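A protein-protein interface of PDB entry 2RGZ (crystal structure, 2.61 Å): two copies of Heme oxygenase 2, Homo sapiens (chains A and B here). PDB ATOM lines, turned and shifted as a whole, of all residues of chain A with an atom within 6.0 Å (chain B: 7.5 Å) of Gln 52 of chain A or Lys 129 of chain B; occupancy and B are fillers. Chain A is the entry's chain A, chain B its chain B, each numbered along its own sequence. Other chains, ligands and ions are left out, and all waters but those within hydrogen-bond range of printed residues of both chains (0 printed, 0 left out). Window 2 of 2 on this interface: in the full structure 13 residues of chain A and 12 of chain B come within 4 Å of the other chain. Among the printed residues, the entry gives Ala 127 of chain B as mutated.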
ATOM      1  N   ASN A  50     -31.249   8.697 -11.555  1.00  0.00           N
ATOM      2  CA  ASN A  50     -30.288   9.128 -10.546  1.00  0.00           C
ATOM      3  C   ASN A  50     -29.316  10.227 -10.934  1.00  0.00           C
ATOM      4  O   ASN A  50     -28.492  10.638 -10.120  1.00  0.00           O
ATOM      5  CB  ASN A  50     -29.512   7.913 -10.050  1.00  0.00           C
ATOM      6  CG  ASN A  50     -30.433   6.815  -9.550  1.00  0.00           C
ATOM      7  OD1 ASN A  50     -31.177   7.008  -8.577  1.00  0.00           O
ATOM      8  ND2 ASN A  50     -30.403   5.663 -10.217  1.00  0.00           N
ATOM      9  N   THR A  51     -29.400  10.719 -12.161  1.00  0.00           N
ATOM     10  CA  THR A  51     -28.480  11.763 -12.559  1.00  0.00           C
ATOM     11  C   THR A  51     -28.774  12.997 -11.688  1.00  0.00           C
ATOM     12  O   THR A  51     -29.929  13.374 -11.497  1.00  0.00           O
ATOM     13  CB  THR A  51     -28.601  12.050 -14.085  1.00  0.00           C
ATOM     14  OG1 THR A  51     -27.383  12.647 -14.549  1.00  0.00           O
ATOM     15  CG2 THR A  51     -29.779  12.978 -14.386  1.00  0.00           C
ATOM     16  N   GLN A  52     -27.727  13.613 -11.148  1.00  0.00           N
ATOM     17  CA  GLN A  52     -27.884  14.758 -10.252  1.00  0.00           C
ATOM     18  C   GLN A  52     -28.809  15.884 -10.707  1.00  0.00           C
ATOM     19  O   GLN A  52     -29.499  16.500  -9.880  1.00  0.00           O
ATOM     20  CB  GLN A  52     -26.520  15.346  -9.890  1.00  0.00           C
ATOM     21  CG  GLN A  52     -26.555  16.236  -8.648  1.00  0.00           C
ATOM     22  CD  GLN A  52     -27.110  15.512  -7.423  1.00  0.00           C
ATOM     23  OE1 GLN A  52     -26.549  14.512  -6.970  1.00  0.00           O
ATOM     24  NE2 GLN A  52     -28.220  16.013  -6.887  1.00  0.00           N
ATOM     25  N   PHE A  53     -28.842  16.167 -12.007  1.00  0.00           N
ATOM     26  CA  PHE A  53     -29.717  17.233 -12.475  1.00  0.00           C
ATOM     27  C   PHE A  53     -31.176  16.848 -12.280  1.00  0.00           C
ATOM     28  O   PHE A  53     -31.998  17.690 -11.932  1.00  0.00           O
ATOM     29  CB  PHE A  53     -29.498  17.556 -13.951  1.00  0.00           C
ATOM     30  CG  PHE A  53     -30.513  18.509 -14.498  1.00  0.00           C
ATOM     31  CD1 PHE A  53     -30.404  19.875 -14.257  1.00  0.00           C
ATOM     32  CD2 PHE A  53     -31.642  18.032 -15.168  1.00  0.00           C
ATOM     33  CE1 PHE A  53     -31.409  20.761 -14.670  1.00  0.00           C
ATOM     34  CE2 PHE A  53     -32.656  18.903 -15.586  1.00  0.00           C
ATOM     35  CZ  PHE A  53     -32.544  20.271 -15.335  1.00  0.00           C
ATOM     36  N   VAL A  54     -31.493  15.581 -12.510  1.00  0.00           N
ATOM     37  CA  VAL A  54     -32.857  15.098 -12.371  1.00  0.00           C
ATOM     38  C   VAL A  54     -33.309  15.074 -10.915  1.00  0.00           C
ATOM     39  O   VAL A  54     -34.430  15.489 -10.606  1.00  0.00           O
ATOM     40  CB  VAL A  54     -33.014  13.684 -12.978  1.00  0.00           C
ATOM     41  CG1 VAL A  54     -34.331  13.056 -12.532  1.00  0.00           C
ATOM     42  CG2 VAL A  54     -32.984  13.775 -14.499  1.00  0.00           C
ATOM     43  N   LYS A  55     -32.447  14.576 -10.033  1.00  0.00           N
ATOM     44  CA  LYS A  55     -32.773  14.506  -8.618  1.00  0.00           C
ATOM     45  C   LYS A  55     -32.917  15.926  -8.047  1.00  0.00           C
ATOM     46  O   LYS A  55     -33.841  16.207  -7.279  1.00  0.00           O
ATOM     47  CB  LYS A  55     -31.687  13.734  -7.835  1.00  0.00           C
ATOM     48  CG  LYS A  55     -31.508  12.256  -8.244  1.00  0.00           C
ATOM     49  CD  LYS A  55     -30.590  11.466  -7.301  1.00  0.00           C
ATOM     50  CE  LYS A  55     -31.305  11.073  -5.986  1.00  0.00           C
ATOM     51  NZ  LYS A  55     -30.588  10.072  -5.097  1.00  0.00           N
ATOM     52  N   ASP A  56     -32.016  16.826  -8.437  1.00  0.00           N
ATOM     53  CA  ASP A  56     -32.075  18.190  -7.932  1.00  0.00           C
ATOM     54  C   ASP A  56     -33.278  18.906  -8.489  1.00  0.00           C
ATOM     55  O   ASP A  56     -33.777  19.863  -7.889  1.00  0.00           O
ATOM     56  CB  ASP A  56     -30.802  18.956  -8.275  1.00  0.00           C
ATOM     57  CG  ASP A  56     -29.617  18.510  -7.436  1.00  0.00           C
ATOM     58  OD1 ASP A  56     -29.837  18.133  -6.258  1.00  0.00           O
ATOM     59  OD2 ASP A  56     -28.464  18.545  -7.937  1.00  0.00           O
ATOM     60  N   PHE A  57     -33.749  18.450  -9.642  1.00  0.00           N
ATOM     61  CA  PHE A  57     -34.927  19.064 -10.225  1.00  0.00           C
ATOM     62  C   PHE A  57     -36.147  18.637  -9.400  1.00  0.00           C
ATOM     63  O   PHE A  57     -36.880  19.466  -8.869  1.00  0.00           O
ATOM     64  CB  PHE A  57     -35.125  18.613 -11.663  1.00  0.00           C
ATOM     65  CG  PHE A  57     -36.393  19.117 -12.268  1.00  0.00           C
ATOM     66  CD1 PHE A  57     -36.511  20.449 -12.646  1.00  0.00           C
ATOM     67  CD2 PHE A  57     -37.489  18.284 -12.401  1.00  0.00           C
ATOM     68  CE1 PHE A  57     -37.708  20.949 -13.148  1.00  0.00           C
ATOM     69  CE2 PHE A  57     -38.693  18.774 -12.901  1.00  0.00           C
ATOM     70  CZ  PHE A  57     -38.800  20.115 -13.276  1.00  0.00           C
ATOM     71  N   LYS A  59     -36.469  17.726  -6.543  1.00  0.00           N
ATOM     72  CA  LYS A  59     -36.516  18.300  -5.199  1.00  0.00           C
ATOM     73  C   LYS A  59     -36.868  19.787  -5.235  1.00  0.00           C
ATOM     74  O   LYS A  59     -37.122  20.398  -4.206  1.00  0.00           O
ATOM     75  CB  LYS A  59     -35.176  18.105  -4.481  1.00  0.00           C
ATOM     76  CG  LYS A  59     -34.881  16.654  -4.112  1.00  0.00           C
ATOM     77  CD  LYS A  59     -33.507  16.475  -3.462  1.00  0.00           C
ATOM     78  CE  LYS A  59     -32.371  16.828  -4.419  1.00  0.00           C
ATOM     79  NZ  LYS A  59     -31.033  16.469  -3.877  1.00  0.00           N
ATOM     80  N   ILE A  62     -33.760  23.423  -8.889  1.00  0.00           N
ATOM     81  CA  ILE A  62     -33.436  24.180 -10.084  1.00  0.00           C
ATOM     82  C   ILE A  62     -34.271  25.445 -10.222  1.00  0.00           C
ATOM     83  O   ILE A  62     -35.502  25.401 -10.205  1.00  0.00           O
ATOM     84  CB  ILE A  62     -33.553  23.281 -11.340  1.00  0.00           C
ATOM     85  CG1 ILE A  62     -32.308  22.387 -11.433  1.00  0.00           C
ATOM     86  CG2 ILE A  62     -33.681  24.133 -12.606  1.00  0.00           C
ATOM     87  CD1 ILE A  62     -32.064  21.521 -10.214  1.00  0.00           C
ATOM     88  N   ASP A 238     -26.348  20.574 -15.379  1.00  0.00           N
ATOM     89  CA  ASP A 238     -25.874  20.542 -13.994  1.00  0.00           C
ATOM     90  C   ASP A 238     -24.710  21.520 -13.815  1.00  0.00           C
ATOM     91  O   ASP A 238     -24.760  22.401 -12.955  1.00  0.00           O
ATOM     92  CB  ASP A 238     -25.421  19.122 -13.629  1.00  0.00           C
ATOM     93  CG  ASP A 238     -24.741  19.044 -12.261  1.00  0.00           C
ATOM     94  OD1 ASP A 238     -25.439  19.178 -11.231  1.00  0.00           O
ATOM     95  OD2 ASP A 238     -23.503  18.849 -12.220  1.00  0.00           O
ATOM     96  N   GLN B 126     -19.531   8.719  -0.409  1.00  0.00           N
ATOM     97  CA  GLN B 126     -20.331   8.653  -1.627  1.00  0.00           C
ATOM     98  C   GLN B 126     -19.496   9.182  -2.785  1.00  0.00           C
ATOM     99  O   GLN B 126     -18.607  10.016  -2.600  1.00  0.00           O
ATOM    100  CB  GLN B 126     -21.623   9.473  -1.502  1.00  0.00           C
ATOM    101  CG  GLN B 126     -22.646   8.874  -0.551  1.00  0.00           C
ATOM    102  CD  GLN B 126     -23.974   9.612  -0.567  1.00  0.00           C
ATOM    103  OE1 GLN B 126     -24.688   9.611  -1.571  1.00  0.00           O
ATOM    104  NE2 GLN B 126     -24.309  10.244   0.547  1.00  0.00           N
ATOM    105  N   ALA B 127     -19.778   8.676  -3.976  1.00  0.00           N
ATOM    106  CA  ALA B 127     -19.060   9.102  -5.157  1.00  0.00           C
ATOM    107  C   ALA B 127     -19.357  10.579  -5.385  1.00  0.00           C
ATOM    108  O   ALA B 127     -20.514  10.971  -5.556  1.00  0.00           O
ATOM    109  CB  ALA B 127     -19.502   8.277  -6.358  1.00  0.00           C
ATOM    110  N   PRO B 128     -18.317  11.424  -5.363  1.00  0.00           N
ATOM    111  CA  PRO B 128     -18.556  12.851  -5.581  1.00  0.00           C
ATOM    112  C   PRO B 128     -19.233  13.077  -6.936  1.00  0.00           C
ATOM    113  O   PRO B 128     -19.081  12.276  -7.860  1.00  0.00           O
ATOM    114  CB  PRO B 128     -17.154  13.460  -5.477  1.00  0.00           C
ATOM    115  CG  PRO B 128     -16.248  12.323  -5.841  1.00  0.00           C
ATOM    116  CD  PRO B 128     -16.884  11.149  -5.165  1.00  0.00           C
ATOM    117  N   LYS B 129     -19.981  14.168  -7.044  1.00  0.00           N
ATOM    118  CA  LYS B 129     -20.730  14.478  -8.254  1.00  0.00           C
ATOM    119  C   LYS B 129     -19.992  14.615  -9.591  1.00  0.00           C
ATOM    120  O   LYS B 129     -20.515  14.192 -10.626  1.00  0.00           O
ATOM    121  CB  LYS B 129     -21.589  15.718  -8.012  1.00  0.00           C
ATOM    122  CG  LYS B 129     -22.776  15.477  -7.088  1.00  0.00           C
ATOM    123  CD  LYS B 129     -22.342  15.240  -5.643  1.00  0.00           C
ATOM    124  CE  LYS B 129     -23.512  15.358  -4.663  1.00  0.00           C
ATOM    125  NZ  LYS B 129     -24.522  14.274  -4.824  1.00  0.00           N
ATOM    126  N   ALA B 130     -18.803  15.207  -9.591  1.00  0.00           N
ATOM    127  CA  ALA B 130     -18.069  15.357 -10.842  1.00  0.00           C
ATOM    128  C   ALA B 130     -17.522  13.993 -11.255  1.00  0.00           C
ATOM    129  O   ALA B 130     -17.147  13.775 -12.418  1.00  0.00           O
ATOM    130  CB  ALA B 130     -16.935  16.367 -10.685  1.00  0.00           C
ATOM    131  N   ALA B 131     -17.489  13.075 -10.294  1.00  0.00           N
ATOM    132  CA  ALA B 131     -17.011  11.730 -10.545  1.00  0.00           C
ATOM    133  C   ALA B 131     -18.179  10.819 -10.927  1.00  0.00           C
ATOM    134  O   ALA B 131     -18.024   9.895 -11.722  1.00  0.00           O
ATOM    135  CB  ALA B 131     -16.286  11.194  -9.306  1.00  0.00           C
ATOM    136  N   GLN B 132     -19.349  11.082 -10.357  1.00  0.00           N
ATOM    137  CA  GLN B 132     -20.529  10.283 -10.655  1.00  0.00           C
ATOM    138  C   GLN B 132     -20.922  10.463 -12.116  1.00  0.00           C
ATOM    139  O   GLN B 132     -21.488   9.560 -12.736  1.00  0.00           O
ATOM    140  CB  GLN B 132     -21.698  10.687  -9.767  1.00  0.00           C
ATOM    141  CG  GLN B 132     -22.905   9.784  -9.949  1.00  0.00           C
ATOM    142  CD  GLN B 132     -22.516   8.313  -9.939  1.00  0.00           C
ATOM    143  OE1 GLN B 132     -21.515   7.932  -9.327  1.00  0.00           O
ATOM    144  NE2 GLN B 132     -23.311   7.479 -10.605  1.00  0.00           N
ATOM    145  N   LYS B 133     -20.629  11.644 -12.648  1.00  0.00           N
ATOM    146  CA  LYS B 133     -20.913  11.947 -14.037  1.00  0.00           C
ATOM    147  C   LYS B 133     -20.000  11.077 -14.897  1.00  0.00           C
ATOM    148  O   LYS B 133     -20.463  10.245 -15.681  1.00  0.00           O
ATOM    149  CB  LYS B 133     -20.628  13.417 -14.333  1.00  0.00           C
ATOM    150  CG  LYS B 133     -21.577  14.394 -13.692  1.00  0.00           C
ATOM    151  CD  LYS B 133     -21.279  15.812 -14.165  1.00  0.00           C
ATOM    152  CE  LYS B 133     -22.420  16.761 -13.830  1.00  0.00           C
ATOM    153  NZ  LYS B 133     -22.176  18.117 -14.371  1.00  0.00           N
ATOM    154  N   TYR B 134     -18.694  11.287 -14.728  1.00  0.00           N
ATOM    155  CA  TYR B 134     -17.669  10.543 -15.459  1.00  0.00           C
ATOM    156  C   TYR B 134     -17.947   9.057 -15.327  1.00  0.00           C
ATOM    157  O   TYR B 134     -17.777   8.299 -16.282  1.00  0.00           O
ATOM    158  CB  TYR B 134     -16.284  10.879 -14.912  1.00  0.00           C
ATOM    159  CG  TYR B 134     -15.142  10.276 -15.692  1.00  0.00           C
ATOM    160  CD1 TYR B 134     -15.299   9.906 -17.023  1.00  0.00           C
ATOM    161  CD2 TYR B 134     -13.874  10.137 -15.117  1.00  0.00           C
ATOM    162  CE1 TYR B 134     -14.230   9.422 -17.770  1.00  0.00           C
ATOM    163  CE2 TYR B 134     -12.793   9.651 -15.858  1.00  0.00           C
ATOM    164  CZ  TYR B 134     -12.978   9.295 -17.188  1.00  0.00           C
ATOM    165  OH  TYR B 134     -11.918   8.814 -17.949  1.00  0.00           O
ATOM    166  N   VAL B 135     -18.384   8.648 -14.139  1.00  0.00           N
ATOM    167  CA  VAL B 135     -18.730   7.254 -13.895  1.00  0.00           C
ATOM    168  C   VAL B 135     -19.918   6.794 -14.738  1.00  0.00           C
ATOM    169  O   VAL B 135     -19.751   5.976 -15.634  1.00  0.00           O
ATOM    170  CB  VAL B 135     -19.064   7.017 -12.425  1.00  0.00           C
ATOM    171  CG1 VAL B 135     -19.832   5.707 -12.262  1.00  0.00           C
ATOM    172  CG2 VAL B 135     -17.786   6.970 -11.627  1.00  0.00           C
ATOM    173  N   GLU B 136     -21.115   7.313 -14.457  1.00  0.00           N
ATOM    174  CA  GLU B 136     -22.309   6.915 -15.214  1.00  0.00           C
ATOM    175  C   GLU B 136     -21.988   6.748 -16.706  1.00  0.00           C
ATOM    176  O   GLU B 136     -22.500   5.839 -17.365  1.00  0.00           O
ATOM    177  CB  GLU B 136     -23.445   7.943 -15.002  1.00  0.00           C
ATOM    178  CG  GLU B 136     -24.201   7.782 -13.661  1.00  0.00           C
ATOM    179  CD  GLU B 136     -25.111   8.983 -13.279  1.00  0.00           C
ATOM    180  OE1 GLU B 136     -24.598  10.121 -13.199  1.00  0.00           O
ATOM    181  OE2 GLU B 136     -26.336   8.792 -13.028  1.00  0.00           O
ATOM    182  N   GLN B 232     -13.504  18.859 -14.574  1.00  0.00           N
ATOM    183  CA  GLN B 232     -14.635  19.092 -13.687  1.00  0.00           C
ATOM    184  C   GLN B 232     -14.328  18.502 -12.317  1.00  0.00           C
ATOM    185  O   GLN B 232     -14.636  19.107 -11.294  1.00  0.00           O
ATOM    186  CB  GLN B 232     -15.921  18.460 -14.243  1.00  0.00           C
ATOM    187  CG  GLN B 232     -17.002  19.474 -14.638  1.00  0.00           C
ATOM    188  CD  GLN B 232     -18.435  18.916 -14.562  1.00  0.00           C
ATOM    189  OE1 GLN B 232     -19.415  19.648 -14.763  1.00  0.00           O
ATOM    190  NE2 GLN B 232     -18.558  17.624 -14.267  1.00  0.00           N
ATOM    191  N   ILE B 233     -13.711  17.323 -12.303  1.00  0.00           N
ATOM    192  CA  ILE B 233     -13.364  16.664 -11.049  1.00  0.00           C
ATOM    193  C   ILE B 233     -12.256  17.399 -10.287  1.00  0.00           C
ATOM    194  O   ILE B 233     -12.281  17.446  -9.057  1.00  0.00           O
ATOM    195  CB  ILE B 233     -12.894  15.198 -11.271  1.00  0.00           C
ATOM    196  CG1 ILE B 233     -14.035  14.348 -11.836  1.00  0.00           C
ATOM    197  CG2 ILE B 233     -12.412  14.595  -9.943  1.00  0.00           C
ATOM    198  CD1 ILE B 233     -13.665  12.901 -12.079  1.00  0.00           C
ATOM    199  N   GLU B 236     -13.367  20.784  -8.867  1.00  0.00           N
ATOM    200  CA  GLU B 236     -14.507  20.435  -8.031  1.00  0.00           C
ATOM    201  C   GLU B 236     -13.898  20.191  -6.654  1.00  0.00           C
ATOM    202  O   GLU B 236     -14.523  20.439  -5.624  1.00  0.00           O
ATOM    203  CB  GLU B 236     -15.178  19.164  -8.552  1.00  0.00           C
ATOM    204  CG  GLU B 236     -16.585  18.897  -8.026  1.00  0.00           C
ATOM    205  CD  GLU B 236     -16.610  18.286  -6.639  1.00  0.00           C
ATOM    206  OE1 GLU B 236     -17.700  17.876  -6.184  1.00  0.00           O
ATOM    207  OE2 GLU B 236     -15.545  18.213  -5.999  1.00  0.00           O
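Of the printed residues of chain B, Gln 52 of chain A touches Lys 129 (3.0 Å). Lys 129 of chain B touches just one residue of chain A: Gln 52. Of the printed residues of chain B, Asn 50 of chain A touches Glu 136. Printed residues of chain B within 4 Å of Thr 51 of chain A: Glu 136 (3.7 Å). Of the printed residues of chain B, Asp 238 of chain A touches Lys 133 (2.6 Å). Ala 127 of chain B touches none of the printed residues of chain A. The nearest residue of chain A that does not touch Lys 129 of chain B is Asp 238 of chain A (5.6 Å).
Among the printed residues, merely in contact across the chains: Thr 51 of chain A with Glu 136 of chain B and Asn 50 of chain A with Glu 136 of chain B.
NZ of Lys 129 of chain B lies within hydrogen-bond range of OE1 of Gln 52 of chain A. OD2 of Asp 238 of chain A lies within salt-bridge range of NZ of Lys 133 of chain B (2.6 Å).
NE2 of Gln 52 of chain A lies within hydrogen-bond range of OD1 of Asp 56 of chain A, 2.7 Å away. NZ of Lys 133 of chain B lies within hydrogen-bond range of OE1 of Gln 232 of chain B.
Among the printed residues, 4 pairs touch across the chains.
No position is printed for both chains.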
